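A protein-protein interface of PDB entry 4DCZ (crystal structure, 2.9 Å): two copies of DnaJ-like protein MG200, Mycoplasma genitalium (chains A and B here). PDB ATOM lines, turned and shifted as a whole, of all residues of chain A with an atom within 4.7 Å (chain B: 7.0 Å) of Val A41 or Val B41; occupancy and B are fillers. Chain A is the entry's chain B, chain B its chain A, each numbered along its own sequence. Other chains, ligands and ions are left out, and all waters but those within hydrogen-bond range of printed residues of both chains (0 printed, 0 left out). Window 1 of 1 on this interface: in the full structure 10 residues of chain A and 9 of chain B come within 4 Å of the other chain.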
ATOM      1  N   SER A  35     -29.700 -33.478 -27.944  1.00  0.00           N
ATOM      2  CA  SER A  35     -29.219 -34.046 -26.682  1.00  0.00           C
ATOM      3  C   SER A  35     -30.192 -35.067 -26.095  1.00  0.00           C
ATOM      4  O   SER A  35     -31.392 -34.993 -26.291  1.00  0.00           O
ATOM      5  CB  SER A  35     -28.857 -32.937 -25.673  1.00  0.00           C
ATOM      6  OG  SER A  35     -29.956 -32.511 -24.906  1.00  0.00           O
ATOM      7  N   GLY A  39     -31.968 -29.752 -22.065  1.00  0.00           N
ATOM      8  CA  GLY A  39     -31.293 -28.768 -21.212  1.00  0.00           C
ATOM      9  C   GLY A  39     -29.993 -29.244 -20.603  1.00  0.00           C
ATOM     10  O   GLY A  39     -29.525 -28.663 -19.633  1.00  0.00           O
ATOM     11  N   GLU A  40     -29.415 -30.296 -21.168  1.00  0.00           N
ATOM     12  CA  GLU A  40     -28.206 -30.918 -20.626  1.00  0.00           C
ATOM     13  C   GLU A  40     -27.469 -31.662 -21.744  1.00  0.00           C
ATOM     14  O   GLU A  40     -28.083 -32.313 -22.560  1.00  0.00           O
ATOM     15  CB  GLU A  40     -28.582 -31.882 -19.518  1.00  0.00           C
ATOM     16  CG  GLU A  40     -27.401 -32.546 -18.827  1.00  0.00           C
ATOM     17  CD  GLU A  40     -27.815 -33.422 -17.607  1.00  0.00           C
ATOM     18  OE1 GLU A  40     -28.881 -33.135 -16.980  1.00  0.00           O
ATOM     19  OE2 GLU A  40     -27.063 -34.387 -17.272  1.00  0.00           O
ATOM     20  N   VAL A  41     -26.157 -31.519 -21.806  1.00  0.00           N
ATOM     21  CA  VAL A  41     -25.338 -32.242 -22.780  1.00  0.00           C
ATOM     22  C   VAL A  41     -24.267 -32.982 -21.987  1.00  0.00           C
ATOM     23  O   VAL A  41     -23.707 -32.408 -21.056  1.00  0.00           O
ATOM     24  CB  VAL A  41     -24.805 -31.312 -23.877  1.00  0.00           C
ATOM     25  CG1 VAL A  41     -23.868 -31.966 -24.763  1.00  0.00           C
ATOM     26  CG2 VAL A  41     -25.950 -30.875 -24.718  1.00  0.00           C
ATOM     27  N   THR A  42     -24.080 -34.277 -22.276  1.00  0.00           N
ATOM     28  CA  THR A  42     -23.049 -35.075 -21.604  1.00  0.00           C
ATOM     29  C   THR A  42     -22.246 -35.771 -22.673  1.00  0.00           C
ATOM     30  O   THR A  42     -22.654 -35.834 -23.837  1.00  0.00           O
ATOM     31  CB  THR A  42     -23.613 -36.145 -20.653  1.00  0.00           C
ATOM     32  OG1 THR A  42     -24.626 -36.862 -21.339  1.00  0.00           O
ATOM     33  CG2 THR A  42     -24.236 -35.551 -19.443  1.00  0.00           C
ATOM     34  N   ALA A  43     -21.108 -36.315 -22.268  1.00  0.00           N
ATOM     35  CA  ALA A  43     -20.180 -36.879 -23.225  1.00  0.00           C
ATOM     36  C   ALA A  43     -20.891 -37.892 -24.077  1.00  0.00           C
ATOM     37  O   ALA A  43     -20.808 -37.849 -25.285  1.00  0.00           O
ATOM     38  CB  ALA A  43     -18.997 -37.493 -22.530  1.00  0.00           C
ATOM     39  N   ASP A  45     -23.550 -37.970 -25.383  1.00  0.00           N
ATOM     40  CA  ASP A  45     -24.256 -37.409 -26.526  1.00  0.00           C
ATOM     41  C   ASP A  45     -23.292 -37.269 -27.691  1.00  0.00           C
ATOM     42  O   ASP A  45     -23.689 -37.452 -28.862  1.00  0.00           O
ATOM     43  CB  ASP A  45     -24.830 -36.032 -26.226  1.00  0.00           C
ATOM     44  CG  ASP A  45     -26.118 -36.067 -25.417  1.00  0.00           C
ATOM     45  OD1 ASP A  45     -27.067 -36.793 -25.818  1.00  0.00           O
ATOM     46  OD2 ASP A  45     -26.197 -35.308 -24.404  1.00  0.00           O
ATOM     47  N   TRP A  46     -22.038 -36.930 -27.390  1.00  0.00           N
ATOM     48  CA  TRP A  46     -20.999 -36.873 -28.421  1.00  0.00           C
ATOM     49  C   TRP A  46     -20.384 -38.251 -28.760  1.00  0.00           C
ATOM     50  O   TRP A  46     -20.028 -38.533 -29.915  1.00  0.00           O
ATOM     51  CB  TRP A  46     -19.852 -36.034 -27.948  1.00  0.00           C
ATOM     52  CG  TRP A  46     -20.094 -34.587 -27.608  1.00  0.00           C
ATOM     53  CD1 TRP A  46     -20.620 -34.111 -26.468  1.00  0.00           C
ATOM     54  CD2 TRP A  46     -19.685 -33.448 -28.369  1.00  0.00           C
ATOM     55  NE1 TRP A  46     -20.581 -32.749 -26.464  1.00  0.00           N
ATOM     56  CE2 TRP A  46     -20.022 -32.316 -27.633  1.00  0.00           C
ATOM     57  CE3 TRP A  46     -19.062 -33.279 -29.620  1.00  0.00           C
ATOM     58  CZ2 TRP A  46     -19.768 -30.996 -28.095  1.00  0.00           C
ATOM     59  CZ3 TRP A  46     -18.798 -31.958 -30.081  1.00  0.00           C
ATOM     60  CH2 TRP A  46     -19.160 -30.844 -29.311  1.00  0.00           C
ATOM     61  N   PHE A  70     -22.786 -29.086 -29.784  1.00  0.00           N
ATOM     62  CA  PHE A  70     -24.146 -28.821 -29.334  1.00  0.00           C
ATOM     63  C   PHE A  70     -24.231 -27.427 -28.753  1.00  0.00           C
ATOM     64  O   PHE A  70     -23.324 -26.978 -28.084  1.00  0.00           O
ATOM     65  CB  PHE A  70     -24.552 -29.784 -28.251  1.00  0.00           C
ATOM     66  CG  PHE A  70     -24.543 -31.205 -28.674  1.00  0.00           C
ATOM     67  CD1 PHE A  70     -25.671 -31.810 -29.124  1.00  0.00           C
ATOM     68  CD2 PHE A  70     -23.425 -31.948 -28.578  1.00  0.00           C
ATOM     69  CE1 PHE A  70     -25.675 -33.137 -29.489  1.00  0.00           C
ATOM     70  CE2 PHE A  70     -23.445 -33.267 -28.943  1.00  0.00           C
ATOM     71  CZ  PHE A  70     -24.582 -33.844 -29.411  1.00  0.00           C
ATOM     72  N   GLY A  74     -29.133 -27.891 -26.914  1.00  0.00           N
ATOM     73  CA  GLY A  74     -28.833 -29.247 -27.241  1.00  0.00           C
ATOM     74  C   GLY A  74     -28.994 -29.555 -28.718  1.00  0.00           C
ATOM     75  O   GLY A  74     -29.116 -30.710 -29.069  1.00  0.00           O
ATOM     76  N   SER B  35     -17.085 -26.174 -17.446  1.00  0.00           N
ATOM     77  CA  SER B  35     -18.389 -26.354 -16.857  1.00  0.00           C
ATOM     78  C   SER B  35     -18.319 -26.895 -15.465  1.00  0.00           C
ATOM     79  O   SER B  35     -17.497 -27.706 -15.142  1.00  0.00           O
ATOM     80  CB  SER B  35     -19.195 -27.334 -17.674  1.00  0.00           C
ATOM     81  OG  SER B  35     -18.419 -28.457 -18.041  1.00  0.00           O
ATOM     82  N   LYS B  36     -19.241 -26.464 -14.644  1.00  0.00           N
ATOM     83  CA  LYS B  36     -19.280 -26.873 -13.251  1.00  0.00           C
ATOM     84  C   LYS B  36     -18.937 -28.331 -13.108  1.00  0.00           C
ATOM     85  O   LYS B  36     -18.041 -28.658 -12.354  1.00  0.00           O
ATOM     86  CB  LYS B  36     -20.676 -26.581 -12.683  1.00  0.00           C
ATOM     87  CG  LYS B  36     -21.025 -27.228 -11.347  1.00  0.00           C
ATOM     88  CD  LYS B  36     -20.530 -26.408 -10.120  1.00  0.00           C
ATOM     89  CE  LYS B  36     -21.349 -26.743  -8.855  1.00  0.00           C
ATOM     90  NZ  LYS B  36     -22.817 -26.494  -9.120  1.00  0.00           N
ATOM     91  N   VAL B  37     -19.657 -29.213 -13.807  1.00  0.00           N
ATOM     92  CA  VAL B  37     -19.302 -30.664 -13.794  1.00  0.00           C
ATOM     93  C   VAL B  37     -18.565 -31.036 -15.078  1.00  0.00           C
ATOM     94  O   VAL B  37     -19.040 -30.709 -16.180  1.00  0.00           O
ATOM     95  CB  VAL B  37     -20.516 -31.609 -13.702  1.00  0.00           C
ATOM     96  CG1 VAL B  37     -20.045 -33.075 -13.707  1.00  0.00           C
ATOM     97  CG2 VAL B  37     -21.375 -31.281 -12.471  1.00  0.00           C
ATOM     98  N   PRO B  38     -17.407 -31.708 -14.953  1.00  0.00           N
ATOM     99  CA  PRO B  38     -16.705 -32.169 -16.158  1.00  0.00           C
ATOM    100  C   PRO B  38     -17.543 -33.184 -16.976  1.00  0.00           C
ATOM    101  O   PRO B  38     -18.207 -34.078 -16.406  1.00  0.00           O
ATOM    102  CB  PRO B  38     -15.408 -32.809 -15.606  1.00  0.00           C
ATOM    103  CG  PRO B  38     -15.686 -33.133 -14.174  1.00  0.00           C
ATOM    104  CD  PRO B  38     -16.710 -32.110 -13.713  1.00  0.00           C
ATOM    105  N   GLY B  39     -17.529 -32.981 -18.304  1.00  0.00           N
ATOM    106  CA  GLY B  39     -18.292 -33.786 -19.282  1.00  0.00           C
ATOM    107  C   GLY B  39     -19.784 -33.529 -19.391  1.00  0.00           C
ATOM    108  O   GLY B  39     -20.473 -34.208 -20.122  1.00  0.00           O
ATOM    109  N   GLU B  40     -20.282 -32.549 -18.660  1.00  0.00           N
ATOM    110  CA  GLU B  40     -21.685 -32.271 -18.614  1.00  0.00           C
ATOM    111  C   GLU B  40     -21.863 -30.784 -18.677  1.00  0.00           C
ATOM    112  O   GLU B  40     -21.430 -30.063 -17.760  1.00  0.00           O
ATOM    113  CB  GLU B  40     -22.264 -32.759 -17.319  1.00  0.00           C
ATOM    114  CG  GLU B  40     -23.688 -32.276 -17.093  1.00  0.00           C
ATOM    115  CD  GLU B  40     -24.379 -32.941 -15.873  1.00  0.00           C
ATOM    116  OE1 GLU B  40     -24.244 -34.195 -15.723  1.00  0.00           O
ATOM    117  OE2 GLU B  40     -25.048 -32.216 -15.076  1.00  0.00           O
ATOM    118  N   VAL B  41     -22.527 -30.321 -19.731  1.00  0.00           N
ATOM    119  CA  VAL B  41     -22.826 -28.924 -19.893  1.00  0.00           C
ATOM    120  C   VAL B  41     -24.345 -28.674 -19.769  1.00  0.00           C
ATOM    121  O   VAL B  41     -25.127 -29.290 -20.456  1.00  0.00           O
ATOM    122  CB  VAL B  41     -22.253 -28.467 -21.202  1.00  0.00           C
ATOM    123  CG1 VAL B  41     -22.464 -26.993 -21.396  1.00  0.00           C
ATOM    124  CG2 VAL B  41     -20.813 -28.766 -21.166  1.00  0.00           C
ATOM    125  N   THR B  42     -24.745 -27.782 -18.861  1.00  0.00           N
ATOM    126  CA  THR B  42     -26.149 -27.517 -18.546  1.00  0.00           C
ATOM    127  C   THR B  42     -26.461 -26.085 -18.943  1.00  0.00           C
ATOM    128  O   THR B  42     -25.584 -25.334 -19.281  1.00  0.00           O
ATOM    129  CB  THR B  42     -26.353 -27.568 -17.050  1.00  0.00           C
ATOM    130  OG1 THR B  42     -25.446 -26.621 -16.455  1.00  0.00           O
ATOM    131  CG2 THR B  42     -26.057 -28.951 -16.505  1.00  0.00           C
ATOM    132  N   ALA B  43     -27.719 -25.689 -18.851  1.00  0.00           N
ATOM    133  CA  ALA B  43     -28.115 -24.342 -19.199  1.00  0.00           C
ATOM    134  C   ALA B  43     -27.391 -23.315 -18.329  1.00  0.00           C
ATOM    135  O   ALA B  43     -26.992 -22.278 -18.840  1.00  0.00           O
ATOM    136  CB  ALA B  43     -29.628 -24.179 -19.097  1.00  0.00           C
ATOM    137  N   SER B  44     -27.157 -23.594 -17.047  1.00  0.00           N
ATOM    138  CA  SER B  44     -26.391 -22.630 -16.242  1.00  0.00           C
ATOM    139  C   SER B  44     -24.992 -22.354 -16.756  1.00  0.00           C
ATOM    140  O   SER B  44     -24.473 -21.261 -16.588  1.00  0.00           O
ATOM    141  CB  SER B  44     -26.242 -23.101 -14.831  1.00  0.00           C
ATOM    142  OG  SER B  44     -27.493 -23.471 -14.410  1.00  0.00           O
ATOM    143  N   ASP B  45     -24.337 -23.338 -17.334  1.00  0.00           N
ATOM    144  CA  ASP B  45     -22.973 -23.097 -17.754  1.00  0.00           C
ATOM    145  C   ASP B  45     -22.974 -21.988 -18.819  1.00  0.00           C
ATOM    146  O   ASP B  45     -22.080 -21.103 -18.832  1.00  0.00           O
ATOM    147  CB  ASP B  45     -22.323 -24.389 -18.249  1.00  0.00           C
ATOM    148  CG  ASP B  45     -22.018 -25.374 -17.108  1.00  0.00           C
ATOM    149  OD1 ASP B  45     -21.370 -24.981 -16.088  1.00  0.00           O
ATOM    150  OD2 ASP B  45     -22.393 -26.569 -17.277  1.00  0.00           O
ATOM    151  N   TRP B  46     -23.994 -22.009 -19.678  1.00  0.00           N
ATOM    152  CA  TRP B  46     -24.089 -20.985 -20.717  1.00  0.00           C
ATOM    153  C   TRP B  46     -24.710 -19.673 -20.222  1.00  0.00           C
ATOM    154  O   TRP B  46     -24.244 -18.595 -20.597  1.00  0.00           O
ATOM    155  CB  TRP B  46     -24.940 -21.432 -21.899  1.00  0.00           C
ATOM    156  CG  TRP B  46     -24.469 -22.569 -22.734  1.00  0.00           C
ATOM    157  CD1 TRP B  46     -24.783 -23.861 -22.555  1.00  0.00           C
ATOM    158  CD2 TRP B  46     -23.722 -22.507 -23.952  1.00  0.00           C
ATOM    159  NE1 TRP B  46     -24.258 -24.631 -23.555  1.00  0.00           N
ATOM    160  CE2 TRP B  46     -23.599 -23.821 -24.431  1.00  0.00           C
ATOM    161  CE3 TRP B  46     -23.126 -21.473 -24.677  1.00  0.00           C
ATOM    162  CZ2 TRP B  46     -22.912 -24.135 -25.603  1.00  0.00           C
ATOM    163  CZ3 TRP B  46     -22.462 -21.777 -25.853  1.00  0.00           C
ATOM    164  CH2 TRP B  46     -22.364 -23.099 -26.305  1.00  0.00           C
ATOM    165  N   PHE B  70     -18.798 -24.695 -25.375  1.00  0.00           N
ATOM    166  CA  PHE B  70     -18.259 -25.772 -24.592  1.00  0.00           C
ATOM    167  C   PHE B  70     -18.061 -26.994 -25.442  1.00  0.00           C
ATOM    168  O   PHE B  70     -18.927 -27.323 -26.263  1.00  0.00           O
ATOM    169  CB  PHE B  70     -19.220 -26.109 -23.511  1.00  0.00           C
ATOM    170  CG  PHE B  70     -19.324 -25.050 -22.492  1.00  0.00           C
ATOM    171  CD1 PHE B  70     -18.364 -24.925 -21.520  1.00  0.00           C
ATOM    172  CD2 PHE B  70     -20.359 -24.191 -22.487  1.00  0.00           C
ATOM    173  CE1 PHE B  70     -18.468 -23.968 -20.537  1.00  0.00           C
ATOM    174  CE2 PHE B  70     -20.435 -23.217 -21.501  1.00  0.00           C
ATOM    175  CZ  PHE B  70     -19.504 -23.118 -20.543  1.00  0.00           C
ATOM    176  N   ASP B  71     -16.927 -27.656 -25.229  1.00  0.00           N
ATOM    177  CA  ASP B  71     -16.507 -28.814 -26.019  1.00  0.00           C
ATOM    178  C   ASP B  71     -16.946 -30.071 -25.310  1.00  0.00           C
ATOM    179  O   ASP B  71     -17.549 -29.977 -24.250  1.00  0.00           O
ATOM    180  CB  ASP B  71     -14.970 -28.804 -26.328  1.00  0.00           C
ATOM    181  CG  ASP B  71     -14.084 -29.205 -25.130  1.00  0.00           C
ATOM    182  OD1 ASP B  71     -14.622 -29.259 -23.988  1.00  0.00           O
ATOM    183  OD2 ASP B  71     -12.844 -29.446 -25.336  1.00  0.00           O
ATOM    184  N   GLU B  72     -16.648 -31.240 -25.871  1.00  0.00           N
ATOM    185  CA  GLU B  72     -17.127 -32.498 -25.288  1.00  0.00           C
ATOM    186  C   GLU B  72     -16.696 -32.601 -23.817  1.00  0.00           C
ATOM    187  O   GLU B  72     -17.476 -32.998 -22.960  1.00  0.00           O
ATOM    188  CB  GLU B  72     -16.600 -33.639 -26.121  1.00  0.00           C
ATOM    189  CG  GLU B  72     -17.009 -35.041 -25.734  1.00  0.00           C
ATOM    190  CD  GLU B  72     -16.261 -36.075 -26.591  1.00  0.00           C
ATOM    191  OE1 GLU B  72     -15.338 -35.613 -27.306  1.00  0.00           O
ATOM    192  OE2 GLU B  72     -16.578 -37.314 -26.575  1.00  0.00           O
ATOM    193  N   GLN B  73     -15.484 -32.151 -23.518  1.00  0.00           N
ATOM    194  CA  GLN B  73     -14.959 -32.145 -22.142  1.00  0.00           C
ATOM    195  C   GLN B  73     -15.691 -31.162 -21.199  1.00  0.00           C
ATOM    196  O   GLN B  73     -15.632 -31.300 -19.979  1.00  0.00           O
ATOM    197  CB  GLN B  73     -13.436 -31.847 -22.131  1.00  0.00           C
ATOM    198  CG  GLN B  73     -12.527 -32.997 -22.696  1.00  0.00           C
ATOM    199  CD  GLN B  73     -12.807 -33.302 -24.203  1.00  0.00           C
ATOM    200  OE1 GLN B  73     -13.133 -34.446 -24.556  1.00  0.00           O
ATOM    201  NE2 GLN B  73     -12.649 -32.291 -25.079  1.00  0.00           N
ATOM    202  N   GLY B  74     -16.377 -30.178 -21.744  1.00  0.00           N
ATOM    203  CA  GLY B  74     -16.865 -29.099 -20.923  1.00  0.00           C
ATOM    204  C   GLY B  74     -15.897 -27.928 -20.879  1.00  0.00           C
ATOM    205  O   GLY B  74     -16.095 -26.967 -20.117  1.00  0.00           O
ATOM    206  N   LYS B  75     -14.852 -27.982 -21.692  1.00  0.00           N
ATOM    207  CA  LYS B  75     -13.931 -26.864 -21.755  1.00  0.00           C
ATOM    208  C   LYS B  75     -14.473 -25.863 -22.715  1.00  0.00           C
ATOM    209  O   LYS B  75     -15.061 -26.223 -23.714  1.00  0.00           O
ATOM    210  CB  LYS B  75     -12.570 -27.306 -22.249  1.00  0.00           C
ATOM    211  CG  LYS B  75     -11.510 -26.232 -22.210  1.00  0.00           C
ATOM    212  CD  LYS B  75     -10.178 -26.821 -22.692  1.00  0.00           C
ATOM    213  CE  LYS B  75      -9.262 -25.757 -23.334  1.00  0.00           C
ATOM    214  NZ  LYS B  75      -7.950 -26.370 -23.699  1.00  0.00           N
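The backbone NH (N) of Ala A43 lies within hydrogen-bond range of the backbone carbonyl oxygen (O) of Gly B39 (3.1 Å).
The backbone NH (N) of Val B41 lies within hydrogen-bond range of the backbone carbonyl oxygen (O) of Val A41, at 2.7 Å.
The side-chain carboxylate (OE2) of Glu A40 sits close to the side-chain carboxylate (OE1) of Glu B40 (3.2 Å).
Gly A39 touches Thr B42, and with the chains exchanged Thr A42 touches Gly B39.
Glu A40 touches Val B41, and with the chains exchanged Val A41 touches Glu B40.
Val A41 touches its own counterpart, Val B41.
Thr A42 touches Glu B40, but with the chains exchanged Glu A40 does not touch Thr B42 (4.5 Å).
OG of Ser B35 sits at hydrogen-bond distance from O of Glu B40 (3.4 Å).
The side-chain hydroxyl (OG) of Ser A35 is in hydrogen-bond range of the backbone carbonyl oxygen (O) of Glu A40, at 3.0 Å.
The backbone NH of Gly B39 is in hydrogen-bond range of the backbone carbonyl oxygen of Gln B73.
The backbone NH (N) of Thr A42 sits at hydrogen-bond distance from the side-chain carboxylate (OD2) of Asp A45, at 3.2 Å.
N of Thr B42 lies within hydrogen-bond range of OD2 of Asp B45 (3.1 Å).
Of the 18 printed residues of chain B, 7 touch a printed residue of chain A.
Of the 10 printed residues of chain A, 7 touch a printed residue of chain B.
Hydrophobic or aromatic side chains of chain A within 4 Å of the printed part of chain B: Val A41 and Trp A46.
Along chain A the printed residues that touch a printed residue of chain B span positions 39 to 70.
O of Gly A39 touches CA of Thr B42, at 3.7 Å.
Ala B43 touches Gly A39 (N to O, 3.6 Å).
Glu A40 touches Val B41.
Val A41 touches Gly B39 (O to O, 3.8 Å).
Val A41 touches Glu B40 (O to CA, 3.2 Å).
Gly B39 touches Thr A42 (O to CA, 3.1 Å).
Thr A42 touches Glu B40 (CG2 to OE1, 3.96 Å).
CG of Trp A46 touches CG of Glu B72, at 3.6 Å.
CZ2 of Trp B46 touches O of Phe A70, 3.8 Å away.
Val A41 touches just these residues of chain B: Gly B39, Glu B40 and Val B41.
Printed residues of chain A within 4 Å of Val B41: Glu A40 (3.5 Å) and Val A41 (2.7 Å).
Of the printed residues of chain B, Gly A39 touches Thr B42 and Ala B43.
Printed residues of chain A within 4 Å of Gly B39: Val A41, Thr A42 and Ala A43.
Printed residues of chain A within 4 Å of Ala B43: Gly A39.
Of the printed residues of chain B, Ala A43 touches Gly B39.
Of the printed residues of chain A, Thr B42 touches Gly A39.
Phe B70 touches none of the printed residues of chain A.
Gln B73 touches none of the printed residues of chain A.
The nearest residue of chain B that does not touch Val A41 is Thr B42 (5.0 Å).
The nearest printed residue of chain B that does not touch Ala A43 is Glu B72 (4.4 Å).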
